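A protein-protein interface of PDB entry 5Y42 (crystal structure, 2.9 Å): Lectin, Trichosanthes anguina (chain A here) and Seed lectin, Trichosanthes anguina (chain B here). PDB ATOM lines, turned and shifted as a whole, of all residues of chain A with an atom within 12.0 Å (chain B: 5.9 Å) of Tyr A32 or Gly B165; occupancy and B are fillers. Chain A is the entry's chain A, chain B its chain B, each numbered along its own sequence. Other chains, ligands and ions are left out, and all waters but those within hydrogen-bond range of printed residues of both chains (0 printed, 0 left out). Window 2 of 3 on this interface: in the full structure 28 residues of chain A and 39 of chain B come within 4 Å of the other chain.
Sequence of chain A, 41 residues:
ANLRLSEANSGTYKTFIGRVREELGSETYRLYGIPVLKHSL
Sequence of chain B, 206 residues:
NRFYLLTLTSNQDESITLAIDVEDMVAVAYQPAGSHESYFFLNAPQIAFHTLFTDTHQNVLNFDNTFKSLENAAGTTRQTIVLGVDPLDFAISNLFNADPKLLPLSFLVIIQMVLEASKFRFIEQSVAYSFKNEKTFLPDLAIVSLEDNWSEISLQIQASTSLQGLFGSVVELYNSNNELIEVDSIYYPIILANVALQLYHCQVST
Among the printed residues, pairs that only touch across the chains: Leu A31 with Gln B158, Tyr A32 with Leu B192, Tyr A32 with Gly B165, Tyr A32 with Thr B161, Tyr A32 with Thr B206, Tyr A32 with Ile B157 and Ile A34 with Ile B157.
The side-chain hydroxyl (OG) of Ser B160 lies within hydrogen-bond range of the side-chain hydroxyl (OH) of Tyr A32 (2.9 Å).
Of the 12 printed residues of chain A, 3 touch a printed residue of chain B.
Printed residues of chain A that touch a printed residue of chain B: Leu A31, Tyr A32 and Ile A34.
Hydrophobic or aromatic side chains of chain A within 4 Å of the printed part of chain B: Leu A31, Tyr A32 and Ile A34.
Of the 16 printed residues of chain B, 7 touch a printed residue of chain A.
Hydrophobic or aromatic side chains of chain B within 4 Å of the printed part of chain A: Ile B157 and Leu B192.
Among the printed residues, 8 pairs touch across the chains.
Tyr A32 touches six residues of chain B.
Of chain A, only Tyr A32 comes within 4 Å of Ser B160.
Thr B161 touches just one residue of chain A: Tyr A32 (3.5 Å).
No residue of chain A comes within 4 Å of Ser B162.
Leu B163 touches none of the printed residues of chain A.
No residue of chain A comes within 4 Å of Gln B164.
No residue of chain A comes within 4 Å of Leu B166.
No residue of chain A comes within 4 Å of Phe B167.
Ser B185 touches none of the printed residues of chain A.
Ile B186 touches none of the printed residues of chain A.
Of the printed residues of chain B, Leu A31 touches Gln B158 (3.3 Å).
Of the printed residues of chain A, Gln B158 touches Leu A31 (3.3 Å).
Printed residues of chain B within 4 Å of Ile A34: Ile B157 (3.9 Å).
Leu A37 touches none of the printed residues of chain B.
The nearest printed residue of chain B that does not touch Ile A34 is Leu B192 (4.1 Å).
The backbone carbonyl oxygen of Ile B157 lies within hydrogen-bond range of the side-chain hydroxyl of Ser B160 (2.6 Å).
The backbone carbonyl oxygen of Ser B160 sits at hydrogen-bond distance from the backbone NH of Gly B165.
OG1 of Thr B161 is in hydrogen-bond range of O of Gln B158, at 2.6 Å.
The backbone carbonyl oxygen (O) of Gly B165 lies within hydrogen-bond range of the backbone NH (N) of Ile B186, at 2.9 Å.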
ATOM      1  N   SER A  26       9.422  15.828   3.542  1.00  0.00           N
ATOM      2  CA  SER A  26       9.229  16.849   2.496  1.00  0.00           C
ATOM      3  C   SER A  26       8.037  17.718   2.833  1.00  0.00           C
ATOM      4  O   SER A  26       6.983  17.257   3.301  1.00  0.00           O
ATOM      5  CB  SER A  26       8.984  16.217   1.147  1.00  0.00           C
ATOM      6  OG  SER A  26       8.682  17.207   0.206  1.00  0.00           O
ATOM      7  N   GLU A  27       8.229  18.994   2.588  1.00  0.00           N
ATOM      8  CA  GLU A  27       7.135  19.998   2.660  1.00  0.00           C
ATOM      9  C   GLU A  27       6.164  19.880   1.501  1.00  0.00           C
ATOM     10  O   GLU A  27       4.957  19.974   1.723  1.00  0.00           O
ATOM     11  CB  GLU A  27       7.706  21.410   2.799  1.00  0.00           C
ATOM     12  CG  GLU A  27       8.310  21.648   4.187  1.00  0.00           C
ATOM     13  CD  GLU A  27       9.203  22.880   4.264  1.00  0.00           C
ATOM     14  OE1 GLU A  27       8.859  23.930   3.678  1.00  0.00           O
ATOM     15  OE2 GLU A  27      10.256  22.799   4.920  1.00  0.00           O
ATOM     16  N   THR A  28       6.655  19.597   0.286  1.00  0.00           N
ATOM     17  CA  THR A  28       5.789  19.496  -0.887  1.00  0.00           C
ATOM     18  C   THR A  28       5.456  18.120  -1.494  1.00  0.00           C
ATOM     19  O   THR A  28       4.491  18.029  -2.228  1.00  0.00           O
ATOM     20  CB  THR A  28       6.318  20.428  -2.002  1.00  0.00           C
ATOM     21  OG1 THR A  28       7.641  20.046  -2.386  1.00  0.00           O
ATOM     22  CG2 THR A  28       6.347  21.875  -1.520  1.00  0.00           C
ATOM     23  N   TYR A  29       6.303  17.122  -1.295  1.00  0.00           N
ATOM     24  CA  TYR A  29       6.126  15.800  -1.915  1.00  0.00           C
ATOM     25  C   TYR A  29       5.493  14.817  -0.928  1.00  0.00           C
ATOM     26  O   TYR A  29       6.155  14.282  -0.030  1.00  0.00           O
ATOM     27  CB  TYR A  29       7.449  15.220  -2.485  1.00  0.00           C
ATOM     28  CG  TYR A  29       7.345  13.939  -3.346  1.00  0.00           C
ATOM     29  CD1 TYR A  29       6.161  13.584  -4.006  1.00  0.00           C
ATOM     30  CD2 TYR A  29       8.447  13.096  -3.512  1.00  0.00           C
ATOM     31  CE1 TYR A  29       6.081  12.440  -4.777  1.00  0.00           C
ATOM     32  CE2 TYR A  29       8.372  11.942  -4.300  1.00  0.00           C
ATOM     33  CZ  TYR A  29       7.185  11.624  -4.937  1.00  0.00           C
ATOM     34  OH  TYR A  29       7.075  10.502  -5.736  1.00  0.00           O
ATOM     35  N   ARG A  30       4.192  14.606  -1.110  1.00  0.00           N
ATOM     36  CA  ARG A  30       3.388  13.700  -0.287  1.00  0.00           C
ATOM     37  C   ARG A  30       2.548  12.778  -1.181  1.00  0.00           C
ATOM     38  O   ARG A  30       2.181  13.063  -2.312  1.00  0.00           O
ATOM     39  CB  ARG A  30       2.477  14.444   0.691  1.00  0.00           C
ATOM     40  CG  ARG A  30       3.146  15.582   1.490  1.00  0.00           C
ATOM     41  CD  ARG A  30       2.184  16.335   2.422  1.00  0.00           C
ATOM     42  NE  ARG A  30       0.845  16.373   1.818  1.00  0.00           N
ATOM     43  CZ  ARG A  30       0.421  17.264   0.915  1.00  0.00           C
ATOM     44  NH1 ARG A  30       1.215  18.276   0.524  1.00  0.00           N
ATOM     45  NH2 ARG A  30      -0.823  17.150   0.411  1.00  0.00           N
ATOM     46  N   LEU A  31       2.264  11.624  -0.638  1.00  0.00           N
ATOM     47  CA  LEU A  31       1.451  10.628  -1.332  1.00  0.00           C
ATOM     48  C   LEU A  31       0.397  10.171  -0.384  1.00  0.00           C
ATOM     49  O   LEU A  31       0.717   9.633   0.655  1.00  0.00           O
ATOM     50  CB  LEU A  31       2.283   9.429  -1.811  1.00  0.00           C
ATOM     51  CG  LEU A  31       3.374   9.616  -2.875  1.00  0.00           C
ATOM     52  CD1 LEU A  31       4.029   8.295  -3.191  1.00  0.00           C
ATOM     53  CD2 LEU A  31       2.860  10.223  -4.161  1.00  0.00           C
ATOM     54  N   TYR A  32      -0.869  10.314  -0.756  1.00  0.00           N
ATOM     55  CA  TYR A  32      -1.981  10.014   0.128  1.00  0.00           C
ATOM     56  C   TYR A  32      -1.834  10.783   1.462  1.00  0.00           C
ATOM     57  O   TYR A  32      -2.273  10.312   2.501  1.00  0.00           O
ATOM     58  CB  TYR A  32      -2.079   8.515   0.386  1.00  0.00           C
ATOM     59  CG  TYR A  32      -2.129   7.632  -0.837  1.00  0.00           C
ATOM     60  CD1 TYR A  32      -3.315   7.455  -1.533  1.00  0.00           C
ATOM     61  CD2 TYR A  32      -1.014   6.910  -1.257  1.00  0.00           C
ATOM     62  CE1 TYR A  32      -3.387   6.617  -2.647  1.00  0.00           C
ATOM     63  CE2 TYR A  32      -1.066   6.070  -2.368  1.00  0.00           C
ATOM     64  CZ  TYR A  32      -2.262   5.917  -3.071  1.00  0.00           C
ATOM     65  OH  TYR A  32      -2.353   5.080  -4.178  1.00  0.00           O
ATOM     66  N   GLY A  33      -1.204  11.965   1.439  1.00  0.00           N
ATOM     67  CA  GLY A  33      -0.962  12.727   2.695  1.00  0.00           C
ATOM     68  C   GLY A  33       0.321  12.428   3.465  1.00  0.00           C
ATOM     69  O   GLY A  33       0.696  13.221   4.347  1.00  0.00           O
ATOM     70  N   ILE A  34       0.994  11.329   3.132  1.00  0.00           N
ATOM     71  CA  ILE A  34       2.204  10.881   3.840  1.00  0.00           C
ATOM     72  C   ILE A  34       3.438  11.453   3.199  1.00  0.00           C
ATOM     73  O   ILE A  34       3.661  11.143   1.988  1.00  0.00           O
ATOM     74  CB  ILE A  34       2.335   9.353   3.715  1.00  0.00           C
ATOM     75  CG1 ILE A  34       1.088   8.628   4.271  1.00  0.00           C
ATOM     76  CG2 ILE A  34       3.610   8.864   4.417  1.00  0.00           C
ATOM     77  CD1 ILE A  34       1.003   7.156   3.879  1.00  0.00           C
ATOM     78  N   PRO A  35       4.219  12.272   3.902  1.00  0.00           N
ATOM     79  CA  PRO A  35       5.472  12.789   3.356  1.00  0.00           C
ATOM     80  C   PRO A  35       6.555  11.782   2.920  1.00  0.00           C
ATOM     81  O   PRO A  35       6.833  10.825   3.618  1.00  0.00           O
ATOM     82  CB  PRO A  35       6.059  13.636   4.492  1.00  0.00           C
ATOM     83  CG  PRO A  35       4.980  13.860   5.439  1.00  0.00           C
ATOM     84  CD  PRO A  35       4.000  12.740   5.279  1.00  0.00           C
ATOM     85  N   VAL A  36       7.142  12.038   1.758  1.00  0.00           N
ATOM     86  CA  VAL A  36       8.346  11.367   1.315  1.00  0.00           C
ATOM     87  C   VAL A  36       9.520  12.073   1.975  1.00  0.00           C
ATOM     88  O   VAL A  36       9.463  13.265   2.180  1.00  0.00           O
ATOM     89  CB  VAL A  36       8.528  11.478  -0.223  1.00  0.00           C
ATOM     90  CG1 VAL A  36       9.801  10.756  -0.672  1.00  0.00           C
ATOM     91  CG2 VAL A  36       7.296  10.924  -0.933  1.00  0.00           C
ATOM     92  N   LEU A  37      10.563  11.322   2.292  1.00  0.00           N
ATOM     93  CA  LEU A  37      11.772  11.905   2.863  1.00  0.00           C
ATOM     94  C   LEU A  37      12.373  12.922   1.911  1.00  0.00           C
ATOM     95  O   LEU A  37      12.334  12.748   0.686  1.00  0.00           O
ATOM     96  CB  LEU A  37      12.818  10.841   3.227  1.00  0.00           C
ATOM     97  CG  LEU A  37      12.516   9.980   4.459  1.00  0.00           C
ATOM     98  CD1 LEU A  37      13.302   8.681   4.485  1.00  0.00           C
ATOM     99  CD2 LEU A  37      12.787  10.780   5.723  1.00  0.00           C
ATOM    100  N   ILE B 157       3.415   1.744  -1.154  1.00  0.00           N
ATOM    101  CA  ILE B 157       2.678   3.022  -1.240  1.00  0.00           C
ATOM    102  C   ILE B 157       2.942   3.737  -2.549  1.00  0.00           C
ATOM    103  O   ILE B 157       2.033   4.161  -3.204  1.00  0.00           O
ATOM    104  CB  ILE B 157       3.055   3.923  -0.049  1.00  0.00           C
ATOM    105  CG1 ILE B 157       2.469   3.311   1.235  1.00  0.00           C
ATOM    106  CG2 ILE B 157       2.494   5.325  -0.239  1.00  0.00           C
ATOM    107  CD1 ILE B 157       2.874   3.981   2.529  1.00  0.00           C
ATOM    108  N   GLN B 158       4.184   3.852  -2.939  1.00  0.00           N
ATOM    109  CA  GLN B 158       4.490   4.478  -4.239  1.00  0.00           C
ATOM    110  C   GLN B 158       3.980   3.676  -5.400  1.00  0.00           C
ATOM    111  O   GLN B 158       3.402   4.256  -6.331  1.00  0.00           O
ATOM    112  CB  GLN B 158       5.979   4.755  -4.330  1.00  0.00           C
ATOM    113  CG  GLN B 158       6.342   5.919  -3.435  1.00  0.00           C
ATOM    114  CD  GLN B 158       7.701   5.774  -2.850  1.00  0.00           C
ATOM    115  OE1 GLN B 158       8.665   5.508  -3.574  1.00  0.00           O
ATOM    116  NE2 GLN B 158       7.800   5.933  -1.522  1.00  0.00           N
ATOM    117  N   SER B 160       1.415   1.753  -5.379  1.00  0.00           N
ATOM    118  CA  SER B 160      -0.044   1.811  -5.347  1.00  0.00           C
ATOM    119  C   SER B 160      -0.664   2.949  -6.110  1.00  0.00           C
ATOM    120  O   SER B 160      -1.826   2.872  -6.482  1.00  0.00           O
ATOM    121  CB  SER B 160      -0.537   1.862  -3.916  1.00  0.00           C
ATOM    122  OG  SER B 160      -0.336   3.160  -3.375  1.00  0.00           O
ATOM    123  N   THR B 161       0.122   3.974  -6.410  1.00  0.00           N
ATOM    124  CA  THR B 161      -0.383   5.106  -7.184  1.00  0.00           C
ATOM    125  C   THR B 161      -0.733   4.733  -8.632  1.00  0.00           C
ATOM    126  O   THR B 161      -1.451   5.446  -9.298  1.00  0.00           O
ATOM    127  CB  THR B 161       0.625   6.266  -7.177  1.00  0.00           C
ATOM    128  OG1 THR B 161       1.872   5.831  -7.732  1.00  0.00           O
ATOM    129  CG2 THR B 161       0.850   6.762  -5.753  1.00  0.00           C
ATOM    130  N   SER B 162      -0.174   3.633  -9.108  1.00  0.00           N
ATOM    131  CA  SER B 162      -0.353   3.123 -10.473  1.00  0.00           C
ATOM    132  C   SER B 162      -1.555   2.225 -10.598  1.00  0.00           C
ATOM    133  O   SER B 162      -1.935   1.865 -11.712  1.00  0.00           O
ATOM    134  CB  SER B 162       0.910   2.380 -10.906  1.00  0.00           C
ATOM    135  OG  SER B 162       1.087   1.199 -10.160  1.00  0.00           O
ATOM    136  N   LEU B 163      -2.152   1.771  -9.498  1.00  0.00           N
ATOM    137  CA  LEU B 163      -3.322   0.899  -9.583  1.00  0.00           C
ATOM    138  C   LEU B 163      -4.301   1.073  -8.434  1.00  0.00           C
ATOM    139  O   LEU B 163      -4.508   0.137  -7.660  1.00  0.00           O
ATOM    140  CB  LEU B 163      -2.835  -0.555  -9.711  1.00  0.00           C
ATOM    141  CG  LEU B 163      -3.857  -1.652 -10.087  1.00  0.00           C
ATOM    142  CD1 LEU B 163      -4.332  -1.518 -11.520  1.00  0.00           C
ATOM    143  CD2 LEU B 163      -3.303  -3.061  -9.877  1.00  0.00           C
ATOM    144  N   GLN B 164      -4.913   2.249  -8.307  1.00  0.00           N
ATOM    145  CA  GLN B 164      -6.075   2.467  -7.439  1.00  0.00           C
ATOM    146  C   GLN B 164      -5.836   2.180  -5.958  1.00  0.00           C
ATOM    147  O   GLN B 164      -6.720   1.746  -5.239  1.00  0.00           O
ATOM    148  CB  GLN B 164      -7.304   1.610  -7.868  1.00  0.00           C
ATOM    149  CG  GLN B 164      -7.839   1.770  -9.277  1.00  0.00           C
ATOM    150  CD  GLN B 164      -8.539   3.089  -9.539  1.00  0.00           C
ATOM    151  OE1 GLN B 164      -8.428   4.086  -8.793  1.00  0.00           O
ATOM    152  NE2 GLN B 164      -9.286   3.095 -10.634  1.00  0.00           N
ATOM    153  N   GLY B 165      -4.607   2.388  -5.503  1.00  0.00           N
ATOM    154  CA  GLY B 165      -4.256   2.222  -4.073  1.00  0.00           C
ATOM    155  C   GLY B 165      -3.998   0.789  -3.677  1.00  0.00           C
ATOM    156  O   GLY B 165      -3.845   0.481  -2.506  1.00  0.00           O
ATOM    157  N   LEU B 166      -3.913  -0.101  -4.649  1.00  0.00           N
ATOM    158  CA  LEU B 166      -3.547  -1.477  -4.383  1.00  0.00           C
ATOM    159  C   LEU B 166      -2.038  -1.689  -4.456  1.00  0.00           C
ATOM    160  O   LEU B 166      -1.355  -1.164  -5.307  1.00  0.00           O
ATOM    161  CB  LEU B 166      -4.184  -2.408  -5.404  1.00  0.00           C
ATOM    162  CG  LEU B 166      -5.696  -2.492  -5.280  1.00  0.00           C
ATOM    163  CD1 LEU B 166      -6.351  -3.098  -6.504  1.00  0.00           C
ATOM    164  CD2 LEU B 166      -6.065  -3.351  -4.086  1.00  0.00           C
ATOM    165  N   PHE B 167      -1.541  -2.488  -3.545  1.00  0.00           N
ATOM    166  CA  PHE B 167      -0.129  -2.808  -3.440  1.00  0.00           C
ATOM    167  C   PHE B 167       0.261  -3.814  -4.512  1.00  0.00           C
ATOM    168  O   PHE B 167      -0.569  -4.558  -4.992  1.00  0.00           O
ATOM    169  CB  PHE B 167       0.222  -3.417  -2.074  1.00  0.00           C
ATOM    170  CG  PHE B 167       0.263  -2.436  -0.908  1.00  0.00           C
ATOM    171  CD1 PHE B 167       0.043  -1.054  -1.058  1.00  0.00           C
ATOM    172  CD2 PHE B 167       0.579  -2.911   0.363  1.00  0.00           C
ATOM    173  CE1 PHE B 167       0.118  -0.198   0.041  1.00  0.00           C
ATOM    174  CE2 PHE B 167       0.642  -2.065   1.452  1.00  0.00           C
ATOM    175  CZ  PHE B 167       0.418  -0.710   1.295  1.00  0.00           C
ATOM    176  N   ASP B 184      -2.620  -5.453   1.625  1.00  0.00           N
ATOM    177  CA  ASP B 184      -2.326  -5.417   0.193  1.00  0.00           C
ATOM    178  C   ASP B 184      -2.894  -4.169  -0.448  1.00  0.00           C
ATOM    179  O   ASP B 184      -3.102  -4.153  -1.677  1.00  0.00           O
ATOM    180  CB  ASP B 184      -2.861  -6.722  -0.426  1.00  0.00           C
ATOM    181  CG  ASP B 184      -4.390  -6.890  -0.254  1.00  0.00           C
ATOM    182  OD1 ASP B 184      -4.851  -7.038   0.927  1.00  0.00           O
ATOM    183  OD2 ASP B 184      -5.119  -6.879  -1.283  1.00  0.00           O
ATOM    184  N   SER B 185      -3.038  -3.088   0.313  1.00  0.00           N
ATOM    185  CA  SER B 185      -3.610  -1.835  -0.192  1.00  0.00           C
ATOM    186  C   SER B 185      -3.362  -0.724   0.780  1.00  0.00           C
ATOM    187  O   SER B 185      -3.048  -0.967   1.911  1.00  0.00           O
ATOM    188  CB  SER B 185      -5.110  -1.947  -0.447  1.00  0.00           C
ATOM    189  OG  SER B 185      -5.847  -1.840   0.740  1.00  0.00           O
ATOM    190  N   ILE B 186      -3.563   0.510   0.344  1.00  0.00           N
ATOM    191  CA  ILE B 186      -3.492   1.659   1.230  1.00  0.00           C
ATOM    192  C   ILE B 186      -4.743   1.841   2.116  1.00  0.00           C
ATOM    193  O   ILE B 186      -4.756   2.625   3.039  1.00  0.00           O
ATOM    194  CB  ILE B 186      -3.218   2.915   0.391  1.00  0.00           C
ATOM    195  CG1 ILE B 186      -2.588   4.016   1.224  1.00  0.00           C
ATOM    196  CG2 ILE B 186      -4.488   3.467  -0.216  1.00  0.00           C
ATOM    197  CD1 ILE B 186      -1.187   3.693   1.681  1.00  0.00           C
ATOM    198  N   TYR B 187      -5.787   1.061   1.895  1.00  0.00           N
ATOM    199  CA  TYR B 187      -7.089   1.325   2.504  1.00  0.00           C
ATOM    200  C   TYR B 187      -7.158   0.617   3.871  1.00  0.00           C
ATOM    201  O   TYR B 187      -8.113  -0.055   4.225  1.00  0.00           O
ATOM    202  CB  TYR B 187      -8.224   0.852   1.583  1.00  0.00           C
ATOM    203  CG  TYR B 187      -8.134   1.471   0.211  1.00  0.00           C
ATOM    204  CD1 TYR B 187      -8.301   2.853   0.040  1.00  0.00           C
ATOM    205  CD2 TYR B 187      -7.832   0.699  -0.907  1.00  0.00           C
ATOM    206  CE1 TYR B 187      -8.185   3.434  -1.204  1.00  0.00           C
ATOM    207  CE2 TYR B 187      -7.718   1.274  -2.164  1.00  0.00           C
ATOM    208  CZ  TYR B 187      -7.896   2.641  -2.303  1.00  0.00           C
ATOM    209  OH  TYR B 187      -7.795   3.245  -3.523  1.00  0.00           O
ATOM    210  N   LEU B 192      -2.124   3.891   6.353  1.00  0.00           N
ATOM    211  CA  LEU B 192      -2.327   5.276   5.984  1.00  0.00           C
ATOM    212  C   LEU B 192      -2.266   6.254   7.155  1.00  0.00           C
ATOM    213  O   LEU B 192      -1.736   7.355   6.997  1.00  0.00           O
ATOM    214  CB  LEU B 192      -3.638   5.470   5.257  1.00  0.00           C
ATOM    215  CG  LEU B 192      -4.014   6.863   4.736  1.00  0.00           C
ATOM    216  CD1 LEU B 192      -3.251   7.277   3.487  1.00  0.00           C
ATOM    217  CD2 LEU B 192      -5.472   6.815   4.405  1.00  0.00           C
ATOM    218  N   THR B 206      -0.152  11.539  -6.469  1.00  0.00           N
ATOM    219  CA  THR B 206      -1.611  11.338  -6.214  1.00  0.00           C
ATOM    220  C   THR B 206      -2.525  12.559  -6.512  1.00  0.00           C
ATOM    221  O   THR B 206      -2.144  13.529  -7.184  1.00  0.00           O
ATOM    222  CB  THR B 206      -1.884  10.901  -4.756  1.00  0.00           C
ATOM    223  OG1 THR B 206      -1.566  11.965  -3.837  1.00  0.00           O
ATOM    224  CG2 THR B 206      -1.096   9.638  -4.411  1.00  0.00           C
